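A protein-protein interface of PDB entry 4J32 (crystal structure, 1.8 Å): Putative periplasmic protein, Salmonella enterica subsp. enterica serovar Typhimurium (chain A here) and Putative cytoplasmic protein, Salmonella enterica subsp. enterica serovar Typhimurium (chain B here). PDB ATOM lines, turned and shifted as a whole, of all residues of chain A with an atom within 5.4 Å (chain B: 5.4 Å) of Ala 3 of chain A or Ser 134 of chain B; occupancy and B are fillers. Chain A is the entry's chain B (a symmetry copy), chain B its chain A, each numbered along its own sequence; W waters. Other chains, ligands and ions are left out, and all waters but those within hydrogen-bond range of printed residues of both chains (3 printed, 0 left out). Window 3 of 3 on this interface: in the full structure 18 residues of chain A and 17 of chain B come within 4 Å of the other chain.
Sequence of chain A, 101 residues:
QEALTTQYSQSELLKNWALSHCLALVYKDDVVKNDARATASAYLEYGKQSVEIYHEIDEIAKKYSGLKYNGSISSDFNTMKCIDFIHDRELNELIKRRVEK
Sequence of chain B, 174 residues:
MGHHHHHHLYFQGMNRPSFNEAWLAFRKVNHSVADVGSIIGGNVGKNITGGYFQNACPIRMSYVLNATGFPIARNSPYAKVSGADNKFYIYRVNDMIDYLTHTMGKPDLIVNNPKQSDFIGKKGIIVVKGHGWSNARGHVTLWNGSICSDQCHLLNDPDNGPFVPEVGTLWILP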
ATOM      1  N   GLN A   1      18.008 -24.087  22.636  1.00  0.00           N
ATOM      2  CA  GLN A   1      18.812 -24.272  23.859  1.00  0.00           C
ATOM      3  C   GLN A   1      18.869 -22.934  24.596  1.00  0.00           C
ATOM      4  O   GLN A   1      19.142 -21.882  24.002  1.00  0.00           O
ATOM      5  CB  GLN A   1      20.206 -24.808  23.484  1.00  0.00           C
ATOM      6  CG  GLN A   1      20.196 -26.308  23.064  1.00  0.00           C
ATOM      7  CD  GLN A   1      20.982 -26.642  21.780  1.00  0.00           C
ATOM      8  OE1 GLN A   1      21.090 -25.832  20.852  1.00  0.00           O
ATOM      9  NE2 GLN A   1      21.494 -27.874  21.717  1.00  0.00           N
ATOM     10  N   GLU A   2      18.563 -22.952  25.895  1.00  0.00           N
ATOM     11  CA  GLU A   2      18.748 -21.712  26.675  1.00  0.00           C
ATOM     12  C   GLU A   2      20.230 -21.593  27.028  1.00  0.00           C
ATOM     13  O   GLU A   2      20.842 -22.589  27.423  1.00  0.00           O
ATOM     14  CB  GLU A   2      17.897 -21.684  27.950  1.00  0.00           C
ATOM     15  CG  GLU A   2      17.954 -20.327  28.654  1.00  0.00           C
ATOM     16  CD  GLU A   2      17.050 -20.219  29.869  1.00  0.00           C
ATOM     17  OE1 GLU A   2      17.477 -19.569  30.846  1.00  0.00           O
ATOM     18  OE2 GLU A   2      15.922 -20.756  29.850  1.00  0.00           O
ATOM     19  N   ALA A   3      20.808 -20.396  26.883  1.00  0.00           N
ATOM     20  CA  ALA A   3      22.206 -20.154  27.254  1.00  0.00           C
ATOM     21  C   ALA A   3      22.387 -20.211  28.763  1.00  0.00           C
ATOM     22  O   ALA A   3      21.412 -20.352  29.517  1.00  0.00           O
ATOM     23  CB  ALA A   3      22.681 -18.807  26.719  1.00  0.00           C
ATOM     24  N   LEU A   4      23.635 -20.100  29.208  1.00  0.00           N
ATOM     25  CA  LEU A   4      23.956 -20.195  30.632  1.00  0.00           C
ATOM     26  C   LEU A   4      23.765 -18.902  31.409  1.00  0.00           C
ATOM     27  O   LEU A   4      24.176 -18.817  32.572  1.00  0.00           O
ATOM     28  CB  LEU A   4      25.389 -20.692  30.821  1.00  0.00           C
ATOM     29  CG  LEU A   4      25.678 -22.042  30.169  1.00  0.00           C
ATOM     30  CD1 LEU A   4      27.171 -22.407  30.362  1.00  0.00           C
ATOM     31  CD2 LEU A   4      24.743 -23.163  30.640  1.00  0.00           C
ATOM     32  N   THR A   5      23.146 -17.901  30.772  1.00  0.00           N
ATOM     33  CA  THR A   5      23.116 -16.537  31.300  1.00  0.00           C
ATOM     34  C   THR A   5      22.691 -16.437  32.777  1.00  0.00           C
ATOM     35  O   THR A   5      23.283 -15.673  33.530  1.00  0.00           O
ATOM     36  CB  THR A   5      22.221 -15.645  30.405  1.00  0.00           C
ATOM     37  OG1 THR A   5      22.461 -16.002  29.025  1.00  0.00           O
ATOM     38  CG2 THR A   5      22.544 -14.145  30.599  1.00  0.00           C
ATOM     39  N   THR A   6      21.689 -17.221  33.168  1.00  0.00           N
ATOM     40  CA  THR A   6      21.139 -17.172  34.536  1.00  0.00           C
ATOM     41  C   THR A   6      22.032 -17.805  35.603  1.00  0.00           C
ATOM     42  O   THR A   6      21.747 -17.682  36.811  1.00  0.00           O
ATOM     43  CB  THR A   6      19.776 -17.869  34.631  1.00  0.00           C
ATOM     44  OG1 THR A   6      19.909 -19.226  34.199  1.00  0.00           O
ATOM     45  CG2 THR A   6      18.734 -17.122  33.786  1.00  0.00           C
ATOM     46  N   GLN A   7      23.101 -18.452  35.173  1.00  0.00           N
ATOM     47  CA  GLN A   7      23.965 -19.176  36.099  1.00  0.00           C
ATOM     48  C   GLN A   7      25.136 -18.332  36.617  1.00  0.00           C
ATOM     49  O   GLN A   7      25.784 -18.706  37.613  1.00  0.00           O
ATOM     50  CB  GLN A   7      24.443 -20.489  35.467  1.00  0.00           C
ATOM     51  CG  GLN A   7      23.318 -21.522  35.318  1.00  0.00           C
ATOM     52  CD  GLN A   7      23.720 -22.754  34.517  1.00  0.00           C
ATOM     53  OE1 GLN A   7      24.829 -23.278  34.655  1.00  0.00           O
ATOM     54  NE2 GLN A   7      22.811 -23.226  33.675  1.00  0.00           N
ATOM     55  N   ALA A  42      22.154  -9.036  27.271  1.00  0.00           N
ATOM     56  CA  ALA A  42      21.685 -10.174  28.076  1.00  0.00           C
ATOM     57  C   ALA A  42      22.336 -10.133  29.464  1.00  0.00           C
ATOM     58  O   ALA A  42      21.672 -10.354  30.493  1.00  0.00           O
ATOM     59  CB  ALA A  42      21.992 -11.499  27.371  1.00  0.00           C
ATOM     60  N   TYR A  46      20.495  -9.136  33.670  1.00  0.00           N
ATOM     61  CA  TYR A  46      20.579  -9.896  34.934  1.00  0.00           C
ATOM     62  C   TYR A  46      21.410  -9.213  36.023  1.00  0.00           C
ATOM     63  O   TYR A  46      21.443  -9.668  37.188  1.00  0.00           O
ATOM     64  CB  TYR A  46      21.095 -11.305  34.652  1.00  0.00           C
ATOM     65  CG  TYR A  46      20.085 -12.169  33.914  1.00  0.00           C
ATOM     66  CD1 TYR A  46      18.997 -12.737  34.585  1.00  0.00           C
ATOM     67  CD2 TYR A  46      20.197 -12.391  32.547  1.00  0.00           C
ATOM     68  CE1 TYR A  46      18.052 -13.549  33.901  1.00  0.00           C
ATOM     69  CE2 TYR A  46      19.247 -13.189  31.852  1.00  0.00           C
ATOM     70  CZ  TYR A  46      18.193 -13.762  32.540  1.00  0.00           C
ATOM     71  OH  TYR A  46      17.278 -14.581  31.871  1.00  0.00           O
ATOM     72  N   GLY B 132      13.873 -20.687  27.891  1.00  0.00           N
ATOM     73  CA  GLY B 132      14.237 -20.839  26.487  1.00  0.00           C
ATOM     74  C   GLY B 132      14.866 -19.603  25.864  1.00  0.00           C
ATOM     75  O   GLY B 132      15.464 -19.697  24.786  1.00  0.00           O
ATOM     76  N   TRP B 133      14.755 -18.461  26.537  1.00  0.00           N
ATOM     77  CA  TRP B 133      15.397 -17.229  26.064  1.00  0.00           C
ATOM     78  C   TRP B 133      16.686 -16.958  26.810  1.00  0.00           C
ATOM     79  O   TRP B 133      16.775 -17.162  28.014  1.00  0.00           O
ATOM     80  CB  TRP B 133      14.504 -16.003  26.223  1.00  0.00           C
ATOM     81  CG  TRP B 133      13.417 -15.873  25.203  1.00  0.00           C
ATOM     82  CD1 TRP B 133      13.347 -16.459  23.962  1.00  0.00           C
ATOM     83  CD2 TRP B 133      12.244 -15.070  25.341  1.00  0.00           C
ATOM     84  NE1 TRP B 133      12.188 -16.048  23.321  1.00  0.00           N
ATOM     85  CE2 TRP B 133      11.496 -15.207  24.151  1.00  0.00           C
ATOM     86  CE3 TRP B 133      11.756 -14.242  26.362  1.00  0.00           C
ATOM     87  CZ2 TRP B 133      10.264 -14.547  23.955  1.00  0.00           C
ATOM     88  CZ3 TRP B 133      10.530 -13.593  26.172  1.00  0.00           C
ATOM     89  CH2 TRP B 133       9.804 -13.749  24.967  1.00  0.00           C
ATOM     90  N   SER B 134      17.668 -16.463  26.072  1.00  0.00           N
ATOM     91  CA  SER B 134      19.014 -16.318  26.580  1.00  0.00           C
ATOM     92  C   SER B 134      19.277 -14.930  27.154  1.00  0.00           C
ATOM     93  O   SER B 134      20.357 -14.704  27.712  1.00  0.00           O
ATOM     94  CB  SER B 134      19.996 -16.608  25.457  1.00  0.00           C
ATOM     95  OG  SER B 134      19.952 -17.991  25.132  1.00  0.00           O
ATOM     96  N   ASN B 135      18.326 -14.019  27.002  1.00  0.00           N
ATOM     97  CA  ASN B 135      18.522 -12.622  27.410  1.00  0.00           C
ATOM     98  C   ASN B 135      17.525 -12.150  28.473  1.00  0.00           C
ATOM     99  O   ASN B 135      17.579 -10.990  28.889  1.00  0.00           O
ATOM    100  CB  ASN B 135      18.428 -11.698  26.180  1.00  0.00           C
ATOM    101  CG  ASN B 135      16.995 -11.626  25.636  1.00  0.00           C
ATOM    102  OD1 ASN B 135      16.351 -12.667  25.428  1.00  0.00           O
ATOM    103  ND2 ASN B 135      16.483 -10.417  25.457  1.00  0.00           N
ATOM    104  N   ALA B 136      16.606 -13.029  28.883  1.00  0.00           N
ATOM    105  CA  ALA B 136      15.498 -12.624  29.757  1.00  0.00           C
ATOM    106  C   ALA B 136      14.739 -13.836  30.276  1.00  0.00           C
ATOM    107  O   ALA B 136      14.806 -14.915  29.694  1.00  0.00           O
ATOM    108  CB  ALA B 136      14.533 -11.669  29.023  1.00  0.00           C
HETATM  109  O   HOH W   1      18.173 -19.618  23.823  1.00  0.00           O
HETATM  110  O   HOH W   2      15.669 -21.984  23.158  1.00  0.00           O
HETATM  111  O   HOH W   3      18.350 -16.069  30.018  1.00  0.00           O
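The backbone carbonyl oxygen (O) of Ser 134 of chain B sits at hydrogen-bond distance from the side-chain hydroxyl (OG1) of Thr 5 of chain A (2.8 Å). The backbone carbonyl oxygen of Ala 136 of chain B sits close to the side-chain hydroxyl of Tyr 46 of chain A, 3.3 Å away. N of Gly 132 of chain B lies within hydrogen-bond range of OE2 of Glu 2 of chain A (2.8 Å). The side-chain hydroxyl (OG) of Ser 134 of chain B is in hydrogen-bond range of the backbone NH (N) of Ala 3 of chain A.
Among the printed residues, pairs that only touch across the chains: Glu 2 of chain A with Trp 133 of chain B, Ala 42 of chain A with Ser 134 of chain B, Ala 42 of chain A with Asn 135 of chain B and Tyr 46 of chain A with Asn 135 of chain B.
Ala 3 of chain A touches one residue of chain B. Of chain A, only Ala 3, Thr 5 and Ala 42 come within 4 Å of Ser 134 of chain B. Printed residues of chain A within 4 Å of Gly 132 of chain B: Glu 2 (2.8 Å). Printed residues of chain A within 4 Å of Trp 133 of chain B: Glu 2. Of the printed residues of chain B, Ala 42 of chain A touches Ser 134 and Asn 135. Printed residues of chain A within 4 Å of Asn 135 of chain B: Ala 42 (3.6 Å) and Tyr 46 (3.9 Å). Gln 1 of chain A touches none of the printed residues of chain B. Leu 4 of chain A touches none of the printed residues of chain B. The nearest residue of chain B that does not touch Ala 3 of chain A is Trp 133 of chain B (5.3 Å). The nearest residue of chain A that does not touch Ser 134 of chain B is Glu 2 of chain A (4.1 Å).
Among the printed residues, 8 pairs touch across the chains. Among the printed residues, no Asp or Glu carboxylate lies within 4 Å of a Lys or Arg side-chain nitrogen of the other chain.
Water W1 lies within hydrogen-bond range of the backbone carbonyl oxygen of Gln 1 of chain A (2.5 Å), the side-chain hydroxyl of Ser 134 of chain B (2.7 Å) and the backbone carbonyl oxygen of Gly 132 of chain B (2.9 Å). Water W3 lies within hydrogen-bond range of OH of Tyr 46 of chain A, O of Trp 133 of chain B and O of Ser 134 of chain B. Water W2 lies within hydrogen-bond range of the backbone carbonyl oxygen of Gly 132 of chain B (2.8 Å) and the backbone NH of Gln 1 of chain A (3.2 Å).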
